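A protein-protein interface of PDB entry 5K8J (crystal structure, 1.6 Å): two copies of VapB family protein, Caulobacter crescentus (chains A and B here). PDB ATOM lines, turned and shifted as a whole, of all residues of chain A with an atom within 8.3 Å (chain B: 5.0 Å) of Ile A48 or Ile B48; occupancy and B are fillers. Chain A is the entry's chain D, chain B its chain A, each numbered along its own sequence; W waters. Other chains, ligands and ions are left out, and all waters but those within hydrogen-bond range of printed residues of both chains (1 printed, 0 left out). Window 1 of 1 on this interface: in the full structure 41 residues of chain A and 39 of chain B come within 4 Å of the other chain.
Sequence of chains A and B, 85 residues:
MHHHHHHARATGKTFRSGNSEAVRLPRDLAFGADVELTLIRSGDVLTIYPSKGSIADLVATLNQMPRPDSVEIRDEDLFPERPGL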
ATOM      1  N   ALA A  10      15.788 -10.841  -3.318  1.00  0.00           N
ATOM      2  CA  ALA A  10      15.080 -12.113  -3.321  1.00  0.00           C
ATOM      3  C   ALA A  10      14.292 -12.220  -4.623  1.00  0.00           C
ATOM      4  O   ALA A  10      14.199 -11.267  -5.400  1.00  0.00           O
ATOM      5  CB  ALA A  10      14.141 -12.232  -2.122  1.00  0.00           C
ATOM      6  N   GLY A  12      10.398 -13.993  -5.995  1.00  0.00           N
ATOM      7  CA  GLY A  12       9.173 -14.620  -5.541  1.00  0.00           C
ATOM      8  C   GLY A  12       8.009 -14.212  -6.411  1.00  0.00           C
ATOM      9  O   GLY A  12       8.136 -13.391  -7.316  1.00  0.00           O
ATOM     10  N   THR A  14       3.684 -13.157  -6.207  1.00  0.00           N
ATOM     11  CA  THR A  14       2.655 -12.675  -5.311  1.00  0.00           C
ATOM     12  C   THR A  14       1.789 -13.846  -4.843  1.00  0.00           C
ATOM     13  O   THR A  14       1.772 -14.918  -5.449  1.00  0.00           O
ATOM     14  CB  THR A  14       1.805 -11.620  -6.010  1.00  0.00           C
ATOM     15  OG1 THR A  14       1.009 -12.237  -7.032  1.00  0.00           O
ATOM     16  CG2 THR A  14       2.708 -10.528  -6.642  1.00  0.00           C
ATOM     17  N   ALA A  22      -0.779  -9.822  -2.464  1.00  0.00           N
ATOM     18  CA  ALA A  22       0.268  -9.370  -1.556  1.00  0.00           C
ATOM     19  C   ALA A  22       1.590 -10.001  -1.969  1.00  0.00           C
ATOM     20  O   ALA A  22       1.632 -10.935  -2.775  1.00  0.00           O
ATOM     21  CB  ALA A  22      -0.051  -9.721  -0.098  1.00  0.00           C
ATOM     22  N   VAL A  23       2.686  -9.475  -1.412  1.00  0.00           N
ATOM     23  CA  VAL A  23       4.007 -10.080  -1.569  1.00  0.00           C
ATOM     24  C   VAL A  23       4.603 -10.295  -0.195  1.00  0.00           C
ATOM     25  O   VAL A  23       4.483  -9.433   0.686  1.00  0.00           O
ATOM     26  CB  VAL A  23       4.978  -9.228  -2.428  1.00  0.00           C
ATOM     27  CG1 VAL A  23       4.543  -9.228  -3.859  1.00  0.00           C
ATOM     28  CG2 VAL A  23       5.101  -7.808  -1.886  1.00  0.00           C
ATOM     29  N   ARG A  24       5.235 -11.454  -0.010  1.00  0.00           N
ATOM     30  CA  ARG A  24       5.982 -11.729   1.208  1.00  0.00           C
ATOM     31  C   ARG A  24       7.355 -11.103   1.090  1.00  0.00           C
ATOM     32  O   ARG A  24       7.941 -11.052   0.005  1.00  0.00           O
ATOM     33  CB  ARG A  24       6.132 -13.230   1.467  1.00  0.00           C
ATOM     34  CG  ARG A  24       4.843 -13.966   1.746  1.00  0.00           C
ATOM     35  CD  ARG A  24       5.107 -15.461   1.938  1.00  0.00           C
ATOM     36  NE  ARG A  24       4.147 -16.268   1.187  1.00  0.00           N
ATOM     37  CZ  ARG A  24       2.926 -16.574   1.614  1.00  0.00           C
ATOM     38  NH1 ARG A  24       2.125 -17.310   0.852  1.00  0.00           N
ATOM     39  NH2 ARG A  24       2.506 -16.151   2.802  1.00  0.00           N
ATOM     40  N   LEU A  25       7.848 -10.597   2.205  1.00  0.00           N
ATOM     41  CA  LEU A  25       9.158  -9.963   2.244  1.00  0.00           C
ATOM     42  C   LEU A  25      10.003 -10.740   3.235  1.00  0.00           C
ATOM     43  O   LEU A  25       9.705 -10.718   4.444  1.00  0.00           O
ATOM     44  CB  LEU A  25       9.054  -8.492   2.648  1.00  0.00           C
ATOM     45  CG  LEU A  25       8.149  -7.619   1.784  1.00  0.00           C
ATOM     46  CD1 LEU A  25       8.161  -6.205   2.297  1.00  0.00           C
ATOM     47  CD2 LEU A  25       8.550  -7.650   0.316  1.00  0.00           C
ATOM     48  N   LEU A  29      14.550  -8.210   3.623  1.00  0.00           N
ATOM     49  CA  LEU A  29      13.862  -7.203   2.831  1.00  0.00           C
ATOM     50  C   LEU A  29      12.753  -6.500   3.595  1.00  0.00           C
ATOM     51  O   LEU A  29      12.256  -5.472   3.120  1.00  0.00           O
ATOM     52  CB  LEU A  29      13.251  -7.825   1.560  1.00  0.00           C
ATOM     53  CG  LEU A  29      14.148  -8.408   0.460  1.00  0.00           C
ATOM     54  CD1 LEU A  29      13.297  -8.844  -0.724  1.00  0.00           C
ATOM     55  CD2 LEU A  29      15.194  -7.422  -0.009  1.00  0.00           C
ATOM     56  N   PHE A  31      10.348  -4.338   6.013  1.00  0.00           N
ATOM     57  CA  PHE A  31      10.288  -3.140   6.819  1.00  0.00           C
ATOM     58  C   PHE A  31       9.830  -3.505   8.226  1.00  0.00           C
ATOM     59  O   PHE A  31       9.361  -4.613   8.487  1.00  0.00           O
ATOM     60  CB  PHE A  31       9.320  -2.127   6.211  1.00  0.00           C
ATOM     61  CG  PHE A  31       9.585  -1.803   4.768  1.00  0.00           C
ATOM     62  CD1 PHE A  31       8.970  -2.532   3.772  1.00  0.00           C
ATOM     63  CD2 PHE A  31      10.401  -0.741   4.411  1.00  0.00           C
ATOM     64  CE1 PHE A  31       9.172  -2.236   2.451  1.00  0.00           C
ATOM     65  CE2 PHE A  31      10.606  -0.433   3.075  1.00  0.00           C
ATOM     66  CZ  PHE A  31       9.988  -1.185   2.098  1.00  0.00           C
ATOM     67  N   VAL A  35       4.899  -0.206   9.953  1.00  0.00           N
ATOM     68  CA  VAL A  35       5.544   0.900   9.251  1.00  0.00           C
ATOM     69  C   VAL A  35       4.612   1.357   8.137  1.00  0.00           C
ATOM     70  O   VAL A  35       4.116   0.538   7.359  1.00  0.00           O
ATOM     71  CB  VAL A  35       6.913   0.476   8.695  1.00  0.00           C
ATOM     72  CG1 VAL A  35       7.543   1.590   7.863  1.00  0.00           C
ATOM     73  CG2 VAL A  35       7.836   0.068   9.820  1.00  0.00           C
ATOM     74  N   GLU A  36       4.329   2.656   8.088  1.00  0.00           N
ATOM     75  CA  GLU A  36       3.520   3.197   7.007  1.00  0.00           C
ATOM     76  C   GLU A  36       4.363   3.258   5.742  1.00  0.00           C
ATOM     77  O   GLU A  36       5.485   3.766   5.763  1.00  0.00           O
ATOM     78  CB  GLU A  36       3.002   4.590   7.351  1.00  0.00           C
ATOM     79  CG  GLU A  36       1.637   4.590   8.022  1.00  0.00           C
ATOM     80  CD  GLU A  36       0.557   4.096   7.081  1.00  0.00           C
ATOM     81  OE1 GLU A  36       0.566   4.511   5.899  1.00  0.00           O
ATOM     82  OE2 GLU A  36      -0.279   3.279   7.514  1.00  0.00           O
ATOM     83  N   LEU A  37       3.819   2.748   4.645  1.00  0.00           N
ATOM     84  CA  LEU A  37       4.554   2.651   3.383  1.00  0.00           C
ATOM     85  C   LEU A  37       3.871   3.422   2.267  1.00  0.00           C
ATOM     86  O   LEU A  37       2.645   3.529   2.210  1.00  0.00           O
ATOM     87  CB  LEU A  37       4.692   1.198   2.940  1.00  0.00           C
ATOM     88  CG  LEU A  37       5.377   0.239   3.897  1.00  0.00           C
ATOM     89  CD1 LEU A  37       5.227  -1.190   3.422  1.00  0.00           C
ATOM     90  CD2 LEU A  37       6.852   0.583   4.085  1.00  0.00           C
ATOM     91  N   THR A  38       4.693   3.928   1.350  1.00  0.00           N
ATOM     92  CA  THR A  38       4.262   4.534   0.107  1.00  0.00           C
ATOM     93  C   THR A  38       4.661   3.584  -1.010  1.00  0.00           C
ATOM     94  O   THR A  38       5.780   3.056  -1.001  1.00  0.00           O
ATOM     95  CB  THR A  38       4.924   5.904  -0.094  1.00  0.00           C
ATOM     96  OG1 THR A  38       4.438   6.803   0.931  1.00  0.00           O
ATOM     97  CG2 THR A  38       4.595   6.451  -1.427  1.00  0.00           C
ATOM     98  N   LEU A  39       3.717   3.304  -1.898  1.00  0.00           N
ATOM     99  CA  LEU A  39       3.908   2.406  -3.025  1.00  0.00           C
ATOM    100  C   LEU A  39       3.678   3.192  -4.300  1.00  0.00           C
ATOM    101  O   LEU A  39       2.678   3.905  -4.419  1.00  0.00           O
ATOM    102  CB  LEU A  39       2.932   1.221  -2.956  1.00  0.00           C
ATOM    103  CG  LEU A  39       3.072   0.199  -1.838  1.00  0.00           C
ATOM    104  CD1 LEU A  39       2.550   0.749  -0.529  1.00  0.00           C
ATOM    105  CD2 LEU A  39       2.306  -1.047  -2.230  1.00  0.00           C
ATOM    106  N   ILE A  40       4.613   3.099  -5.247  1.00  0.00           N
ATOM    107  CA  ILE A  40       4.454   3.743  -6.546  1.00  0.00           C
ATOM    108  C   ILE A  40       4.839   2.742  -7.634  1.00  0.00           C
ATOM    109  O   ILE A  40       5.973   2.248  -7.660  1.00  0.00           O
ATOM    110  CB  ILE A  40       5.295   5.022  -6.680  1.00  0.00           C
ATOM    111  CG1 ILE A  40       5.092   5.605  -8.078  1.00  0.00           C
ATOM    112  CG2 ILE A  40       6.749   4.771  -6.333  1.00  0.00           C
ATOM    113  CD1 ILE A  40       5.797   6.895  -8.311  1.00  0.00           C
ATOM    114  N   ARG A  41       3.917   2.470  -8.538  1.00  0.00           N
ATOM    115  CA  ARG A  41       4.154   1.579  -9.668  1.00  0.00           C
ATOM    116  C   ARG A  41       4.144   2.416 -10.935  1.00  0.00           C
ATOM    117  O   ARG A  41       3.204   3.181 -11.163  1.00  0.00           O
ATOM    118  CB  ARG A  41       3.080   0.491  -9.732  1.00  0.00           C
ATOM    119  CG  ARG A  41       3.066  -0.343 -11.009  1.00  0.00           C
ATOM    120  CD  ARG A  41       3.689  -1.669 -10.849  1.00  0.00           C
ATOM    121  NE  ARG A  41       3.772  -2.360 -12.139  1.00  0.00           N
ATOM    122  CZ  ARG A  41       3.066  -3.418 -12.506  1.00  0.00           C
ATOM    123  NH1 ARG A  41       3.253  -3.918 -13.723  1.00  0.00           N
ATOM    124  NH2 ARG A  41       2.206  -4.007 -11.673  1.00  0.00           N
ATOM    125  N   SER A  42       5.192   2.288 -11.743  1.00  0.00           N
ATOM    126  CA  SER A  42       5.287   2.999 -13.013  1.00  0.00           C
ATOM    127  C   SER A  42       5.792   2.007 -14.049  1.00  0.00           C
ATOM    128  O   SER A  42       6.971   1.654 -14.051  1.00  0.00           O
ATOM    129  CB  SER A  42       6.232   4.207 -12.949  1.00  0.00           C
ATOM    130  OG  SER A  42       5.874   5.126 -11.920  1.00  0.00           O
ATOM    131  N   GLY A  43       4.900   1.526 -14.901  1.00  0.00           N
ATOM    132  CA  GLY A  43       5.319   0.530 -15.867  1.00  0.00           C
ATOM    133  C   GLY A  43       5.685  -0.776 -15.188  1.00  0.00           C
ATOM    134  O   GLY A  43       4.870  -1.370 -14.486  1.00  0.00           O
ATOM    135  N   ASP A  44       6.919  -1.237 -15.394  1.00  0.00           N
ATOM    136  CA  ASP A  44       7.357  -2.512 -14.835  1.00  0.00           C
ATOM    137  C   ASP A  44       7.777  -2.419 -13.374  1.00  0.00           C
ATOM    138  O   ASP A  44       7.994  -3.460 -12.735  1.00  0.00           O
ATOM    139  CB  ASP A  44       8.567  -3.053 -15.596  1.00  0.00           C
ATOM    140  CG  ASP A  44       8.270  -3.426 -17.039  1.00  0.00           C
ATOM    141  OD1 ASP A  44       7.176  -3.960 -17.301  1.00  0.00           O
ATOM    142  OD2 ASP A  44       9.151  -3.167 -17.902  1.00  0.00           O
ATOM    143  N   VAL A  45       7.929  -1.214 -12.838  1.00  0.00           N
ATOM    144  CA  VAL A  45       8.664  -1.033 -11.593  1.00  0.00           C
ATOM    145  C   VAL A  45       7.712  -0.617 -10.495  1.00  0.00           C
ATOM    146  O   VAL A  45       7.050   0.418 -10.610  1.00  0.00           O
ATOM    147  CB  VAL A  45       9.766   0.015 -11.751  1.00  0.00           C
ATOM    148  CG1 VAL A  45      10.553   0.141 -10.440  1.00  0.00           C
ATOM    149  CG2 VAL A  45      10.687  -0.362 -12.899  1.00  0.00           C
ATOM    150  N   LEU A  46       7.711  -1.371  -9.405  1.00  0.00           N
ATOM    151  CA  LEU A  46       7.026  -1.003  -8.176  1.00  0.00           C
ATOM    152  C   LEU A  46       8.091  -0.610  -7.155  1.00  0.00           C
ATOM    153  O   LEU A  46       8.996  -1.391  -6.871  1.00  0.00           O
ATOM    154  CB  LEU A  46       6.206  -2.170  -7.645  1.00  0.00           C
ATOM    155  CG  LEU A  46       5.595  -2.037  -6.250  1.00  0.00           C
ATOM    156  CD1 LEU A  46       4.676  -0.846  -6.177  1.00  0.00           C
ATOM    157  CD2 LEU A  46       4.881  -3.315  -5.900  1.00  0.00           C
ATOM    158  N   THR A  47       7.984   0.597  -6.604  1.00  0.00           N
ATOM    159  CA  THR A  47       8.897   1.071  -5.579  1.00  0.00           C
ATOM    160  C   THR A  47       8.124   1.276  -4.280  1.00  0.00           C
ATOM    161  O   THR A  47       7.019   1.834  -4.298  1.00  0.00           O
ATOM    162  CB  THR A  47       9.560   2.383  -6.026  1.00  0.00           C
ATOM    163  OG1 THR A  47      10.191   2.178  -7.302  1.00  0.00           O
ATOM    164  CG2 THR A  47      10.580   2.860  -5.021  1.00  0.00           C
ATOM    165  N   ILE A  48       8.702   0.808  -3.173  1.00  0.00           N
ATOM    166  CA  ILE A  48       8.077   0.885  -1.853  1.00  0.00           C
ATOM    167  C   ILE A  48       9.079   1.515  -0.892  1.00  0.00           C
ATOM    168  O   ILE A  48      10.241   1.093  -0.837  1.00  0.00           O
ATOM    169  CB  ILE A  48       7.629  -0.498  -1.347  1.00  0.00           C
ATOM    170  CG1 ILE A  48       6.787  -1.215  -2.412  1.00  0.00           C
ATOM    171  CG2 ILE A  48       6.850  -0.353  -0.019  1.00  0.00           C
ATOM    172  CD1 ILE A  48       6.269  -2.581  -1.959  1.00  0.00           C
ATOM    173  N   TYR A  49       8.629   2.498  -0.104  1.00  0.00           N
ATOM    174  CA  TYR A  49       9.517   3.133   0.856  1.00  0.00           C
ATOM    175  C   TYR A  49       8.698   3.689   2.018  1.00  0.00           C
ATOM    176  O   TYR A  49       7.479   3.852   1.894  1.00  0.00           O
ATOM    177  CB  TYR A  49      10.341   4.241   0.177  1.00  0.00           C
ATOM    178  CG  TYR A  49       9.546   5.334  -0.503  1.00  0.00           C
ATOM    179  CD1 TYR A  49       9.293   5.307  -1.876  1.00  0.00           C
ATOM    180  CD2 TYR A  49       9.051   6.415   0.226  1.00  0.00           C
ATOM    181  CE1 TYR A  49       8.581   6.311  -2.501  1.00  0.00           C
ATOM    182  CE2 TYR A  49       8.313   7.426  -0.394  1.00  0.00           C
ATOM    183  CZ  TYR A  49       8.091   7.374  -1.755  1.00  0.00           C
ATOM    184  OH  TYR A  49       7.371   8.363  -2.387  1.00  0.00           O
ATOM    185  N   PRO A  50       9.334   3.987   3.153  1.00  0.00           N
ATOM    186  CA  PRO A  50       8.569   4.488   4.310  1.00  0.00           C
ATOM    187  C   PRO A  50       7.990   5.863   4.037  1.00  0.00           C
ATOM    188  O   PRO A  50       8.675   6.758   3.550  1.00  0.00           O
ATOM    189  CB  PRO A  50       9.601   4.519   5.438  1.00  0.00           C
ATOM    190  CG  PRO A  50      10.624   3.490   5.021  1.00  0.00           C
ATOM    191  CD  PRO A  50      10.711   3.637   3.538  1.00  0.00           C
ATOM    192  N   SER A  51       6.707   6.038   4.379  1.00  0.00           N
ATOM    193  CA  SER A  51       6.070   7.328   4.133  1.00  0.00           C
ATOM    194  C   SER A  51       6.652   8.450   4.992  1.00  0.00           C
ATOM    195  O   SER A  51       6.565   9.619   4.589  1.00  0.00           O
ATOM    196  CB  SER A  51       4.575   7.240   4.418  1.00  0.00           C
ATOM    197  OG  SER A  51       3.980   6.245   3.608  1.00  0.00           O
ATOM    198  N   VAL B  23       3.139  -7.394   2.342  1.00  0.00           N
ATOM    199  CA  VAL B  23       2.672  -6.071   1.942  1.00  0.00           C
ATOM    200  C   VAL B  23       1.573  -6.262   0.908  1.00  0.00           C
ATOM    201  O   VAL B  23       1.768  -6.959  -0.095  1.00  0.00           O
ATOM    202  CB  VAL B  23       3.810  -5.198   1.363  1.00  0.00           C
ATOM    203  CG1 VAL B  23       3.273  -3.835   0.894  1.00  0.00           C
ATOM    204  CG2 VAL B  23       4.889  -4.998   2.391  1.00  0.00           C
ATOM    205  N   LEU B  25      -0.789  -5.435  -2.185  1.00  0.00           N
ATOM    206  CA  LEU B  25      -0.661  -4.707  -3.440  1.00  0.00           C
ATOM    207  C   LEU B  25      -2.041  -4.382  -3.993  1.00  0.00           C
ATOM    208  O   LEU B  25      -2.749  -5.291  -4.459  1.00  0.00           O
ATOM    209  CB  LEU B  25       0.141  -5.515  -4.457  1.00  0.00           C
ATOM    210  CG  LEU B  25       1.558  -5.889  -4.016  1.00  0.00           C
ATOM    211  CD1 LEU B  25       2.305  -6.521  -5.194  1.00  0.00           C
ATOM    212  CD2 LEU B  25       2.319  -4.647  -3.490  1.00  0.00           C
ATOM    213  N   PHE B  31       0.952  -7.189  -9.680  1.00  0.00           N
ATOM    214  CA  PHE B  31       1.507  -7.945 -10.794  1.00  0.00           C
ATOM    215  C   PHE B  31       0.667  -9.195 -11.007  1.00  0.00           C
ATOM    216  O   PHE B  31      -0.036  -9.654 -10.107  1.00  0.00           O
ATOM    217  CB  PHE B  31       2.959  -8.360 -10.524  1.00  0.00           C
ATOM    218  CG  PHE B  31       3.931  -7.215 -10.483  1.00  0.00           C
ATOM    219  CD1 PHE B  31       4.253  -6.604  -9.280  1.00  0.00           C
ATOM    220  CD2 PHE B  31       4.540  -6.761 -11.644  1.00  0.00           C
ATOM    221  CE1 PHE B  31       5.160  -5.544  -9.240  1.00  0.00           C
ATOM    222  CE2 PHE B  31       5.446  -5.706 -11.620  1.00  0.00           C
ATOM    223  CZ  PHE B  31       5.746  -5.091 -10.417  1.00  0.00           C
ATOM    224  N   LEU B  37       8.902 -12.315  -9.715  1.00  0.00           N
ATOM    225  CA  LEU B  37       9.360 -10.967  -9.419  1.00  0.00           C
ATOM    226  C   LEU B  37      10.747 -11.016  -8.810  1.00  0.00           C
ATOM    227  O   LEU B  37      11.109 -11.962  -8.096  1.00  0.00           O
ATOM    228  CB  LEU B  37       8.429 -10.252  -8.433  1.00  0.00           C
ATOM    229  CG  LEU B  37       6.969 -10.178  -8.887  1.00  0.00           C
ATOM    230  CD1 LEU B  37       6.102  -9.622  -7.777  1.00  0.00           C
ATOM    231  CD2 LEU B  37       6.836  -9.353 -10.100  1.00  0.00           C
ATOM    232  N   THR B  38      11.510  -9.978  -9.113  1.00  0.00           N
ATOM    233  CA  THR B  38      12.748  -9.663  -8.432  1.00  0.00           C
ATOM    234  C   THR B  38      12.473  -8.538  -7.432  1.00  0.00           C
ATOM    235  O   THR B  38      11.815  -7.546  -7.767  1.00  0.00           O
ATOM    236  CB  THR B  38      13.813  -9.245  -9.450  1.00  0.00           C
ATOM    237  OG1 THR B  38      14.201 -10.394 -10.223  1.00  0.00           O
ATOM    238  CG2 THR B  38      15.021  -8.696  -8.751  1.00  0.00           C
ATOM    239  N   LEU B  39      12.959  -8.709  -6.212  1.00  0.00           N
ATOM    240  CA  LEU B  39      12.778  -7.768  -5.111  1.00  0.00           C
ATOM    241  C   LEU B  39      14.160  -7.369  -4.625  1.00  0.00           C
ATOM    242  O   LEU B  39      14.933  -8.220  -4.183  1.00  0.00           O
ATOM    243  CB  LEU B  39      11.989  -8.399  -3.964  1.00  0.00           C
ATOM    244  CG  LEU B  39      10.568  -8.866  -4.290  1.00  0.00           C
ATOM    245  CD1 LEU B  39      10.573 -10.273  -4.834  1.00  0.00           C
ATOM    246  CD2 LEU B  39       9.726  -8.793  -3.017  1.00  0.00           C
ATOM    247  N   ASP B  44      16.258   1.817   2.735  1.00  0.00           N
ATOM    248  CA  ASP B  44      14.847   1.668   3.052  1.00  0.00           C
ATOM    249  C   ASP B  44      13.974   1.664   1.818  1.00  0.00           C
ATOM    250  O   ASP B  44      12.755   1.816   1.939  1.00  0.00           O
ATOM    251  CB  ASP B  44      14.393   2.797   3.969  1.00  0.00           C
ATOM    252  CG  ASP B  44      14.928   2.651   5.362  1.00  0.00           C
ATOM    253  OD1 ASP B  44      15.282   1.513   5.738  1.00  0.00           O
ATOM    254  OD2 ASP B  44      14.985   3.670   6.081  1.00  0.00           O
ATOM    255  N   VAL B  45      14.563   1.522   0.632  1.00  0.00           N
ATOM    256  CA  VAL B  45      13.816   1.538  -0.618  1.00  0.00           C
ATOM    257  C   VAL B  45      13.806   0.135  -1.211  1.00  0.00           C
ATOM    258  O   VAL B  45      14.863  -0.459  -1.468  1.00  0.00           O
ATOM    259  CB  VAL B  45      14.402   2.542  -1.615  1.00  0.00           C
ATOM    260  CG1 VAL B  45      13.592   2.576  -2.888  1.00  0.00           C
ATOM    261  CG2 VAL B  45      14.439   3.929  -0.990  1.00  0.00           C
ATOM    262  N   LEU B  46      12.607  -0.374  -1.462  1.00  0.00           N
ATOM    263  CA  LEU B  46      12.421  -1.683  -2.063  1.00  0.00           C
ATOM    264  C   LEU B  46      11.941  -1.507  -3.491  1.00  0.00           C
ATOM    265  O   LEU B  46      10.986  -0.766  -3.740  1.00  0.00           O
ATOM    266  CB  LEU B  46      11.399  -2.475  -1.251  1.00  0.00           C
ATOM    267  CG  LEU B  46      11.047  -3.871  -1.732  1.00  0.00           C
ATOM    268  CD1 LEU B  46      12.249  -4.778  -1.609  1.00  0.00           C
ATOM    269  CD2 LEU B  46       9.878  -4.379  -0.866  1.00  0.00           C
ATOM    270  N   THR B  47      12.616  -2.167  -4.442  1.00  0.00           N
ATOM    271  CA  THR B  47      12.284  -2.072  -5.858  1.00  0.00           C
ATOM    272  C   THR B  47      11.896  -3.461  -6.352  1.00  0.00           C
ATOM    273  O   THR B  47      12.635  -4.426  -6.124  1.00  0.00           O
ATOM    274  CB  THR B  47      13.473  -1.532  -6.657  1.00  0.00           C
ATOM    275  OG1 THR B  47      13.833  -0.239  -6.178  1.00  0.00           O
ATOM    276  CG2 THR B  47      13.132  -1.413  -8.132  1.00  0.00           C
ATOM    277  N   ILE B  48      10.749  -3.553  -7.017  1.00  0.00           N
ATOM    278  CA  ILE B  48      10.146  -4.832  -7.402  1.00  0.00           C
ATOM    279  C   ILE B  48       9.791  -4.769  -8.885  1.00  0.00           C
ATOM    280  O   ILE B  48       9.218  -3.776  -9.343  1.00  0.00           O
ATOM    281  CB  ILE B  48       8.892  -5.110  -6.543  1.00  0.00           C
ATOM    282  CG1 ILE B  48       9.265  -5.127  -5.061  1.00  0.00           C
ATOM    283  CG2 ILE B  48       8.249  -6.434  -6.939  1.00  0.00           C
ATOM    284  CD1 ILE B  48       8.072  -5.320  -4.119  1.00  0.00           C
ATOM    285  N   TYR B  49      10.193  -5.783  -9.655  1.00  0.00           N
ATOM    286  CA  TYR B  49       9.937  -5.772 -11.092  1.00  0.00           C
ATOM    287  C   TYR B  49       9.962  -7.212 -11.594  1.00  0.00           C
ATOM    288  O   TYR B  49      10.426  -8.117 -10.890  1.00  0.00           O
ATOM    289  CB  TYR B  49      10.959  -4.901 -11.849  1.00  0.00           C
ATOM    290  CG  TYR B  49      12.387  -5.284 -11.662  1.00  0.00           C
ATOM    291  CD1 TYR B  49      12.983  -6.223 -12.509  1.00  0.00           C
ATOM    292  CD2 TYR B  49      13.149  -4.747 -10.645  1.00  0.00           C
ATOM    293  CE1 TYR B  49      14.298  -6.621 -12.334  1.00  0.00           C
ATOM    294  CE2 TYR B  49      14.480  -5.139 -10.463  1.00  0.00           C
ATOM    295  CZ  TYR B  49      15.042  -6.062 -11.324  1.00  0.00           C
ATOM    296  OH  TYR B  49      16.347  -6.465 -11.166  1.00  0.00           O
ATOM    297  N   PRO B  50       9.479  -7.455 -12.811  1.00  0.00           N
ATOM    298  CA  PRO B  50       9.411  -8.836 -13.314  1.00  0.00           C
ATOM    299  C   PRO B  50      10.803  -9.398 -13.555  1.00  0.00           C
ATOM    300  O   PRO B  50      11.646  -8.747 -14.176  1.00  0.00           O
ATOM    301  CB  PRO B  50       8.632  -8.694 -14.625  1.00  0.00           C
ATOM    302  CG  PRO B  50       7.836  -7.464 -14.449  1.00  0.00           C
ATOM    303  CD  PRO B  50       8.731  -6.530 -13.678  1.00  0.00           C
HETATM  304  O   HOH W   1      12.905   2.091  -7.368  1.00  0.00           O
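Water W1 bridges OG1 of Thr A47 and OG1 of Thr B47.
N of Val B23 is in hydrogen-bond range of O of Val A23 (3.0 Å). The backbone carbonyl oxygen (O) of Gly A12 sits at hydrogen-bond distance from the backbone NH (N) of Leu B37. The backbone NH of Ala A10 is in hydrogen-bond range of the backbone carbonyl oxygen of Leu B39. The backbone NH (N) of Ile A48 is in hydrogen-bond range of the backbone carbonyl oxygen (O) of Leu B46, at 2.8 Å. The backbone NH (N) of Ile B48 lies within hydrogen-bond range of the backbone carbonyl oxygen (O) of Leu A46.
Of chain B, only Asp B44, Val B45, Leu B46 and Ile B48 come within 4 Å of Ile A48. Printed residues of chain A within 4 Å of Ile B48: Asp A44, Val A45, Leu A46 and Ile A48. Printed residues of chain A within 4 Å of Val B23: Ala A22, Val A23, Leu A25 and Leu A37. Of the printed residues of chain B, Pro A50 touches Asp B44 (3.2 Å). Arg A24 touches none of the printed residues of chain B. The nearest residue of chain A that does not touch Ile B48 is Val A23 (4.5 Å). The nearest printed residue of chain A that does not touch Leu B46 is Leu A29 (4.3 Å).
Val A23 touches its own counterpart, Val B23. Asp A44 touches Ile B48, and with the chains exchanged Ile A48 touches Asp B44. Leu A46 touches Thr B47, and with the chains exchanged Thr A47 touches Leu B46. Of the 36 pairs that touch across the chains among the printed residues, 27 have their exchanged pair printed and touching as well.
The backbone carbonyl oxygen (O) of Tyr B49 lies within hydrogen-bond range of the backbone NH (N) of Thr B38 (2.8 Å). N of Thr A38 lies within hydrogen-bond range of O of Tyr A49, at 2.8 Å. O of Ile A40 lies within hydrogen-bond range of N of Thr A47 (2.8 Å). The guanidinium group of Arg A41 is in hydrogen-bond range of the backbone carbonyl oxygen of Gly A43 (2.8 Å).
Among the printed residues, merely in contact across the chains: Ala A10 with Thr B38, Gly A12 with Leu B39, Thr A14 with Leu B37, Ala A22 with Val B23, Val A23 with Leu B25, Leu A25 with Val B23, Leu A25 with Leu B39, Leu A25 with Leu B46, Leu A29 with Leu B39, Phe A31 with Asp B44, Phe A31 with Leu B46, Leu A37 with Val B23, Leu A39 with Leu B25, Arg A41 with Phe B31, Asp A44 with Phe B31, Asp A44 with Ile B48, Asp A44 with Tyr B49, Asp A44 with Pro B50, Val A45 with Thr B47, Val A45 with Ile B48, Leu A46 with Leu B25, Leu A46 with Phe B31, Leu A46 with Leu B46, Leu A46 with Thr B47, Thr A47 with Val B45, Thr A47 with Leu B46, Ile A48 with Asp B44, Ile A48 with Val B45, Ile A48 with Ile B48, Tyr A49 with Asp B44 and Pro A50 with Asp B44.
Printed residues of chain A that touch a printed residue of chain B: Ala A10, Gly A12, Thr A14, Ala A22, Val A23, Leu A25, Leu A29, Phe A31, Leu A37, Leu A39, Arg A41, Asp A44, Val A45, Leu A46, Thr A47, Ile A48, Tyr A49 and Pro A50. Hydrophobic or aromatic side chains of chain A that line the printed part of chain B: Ala A22, Val A23, Leu A25, Leu A29, Phe A31, Leu A37, Leu A39, Val A45, Leu A46, Ile A48, Tyr A49 and Pro A50. Among the printed residues, 36 pairs touch across the chains.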
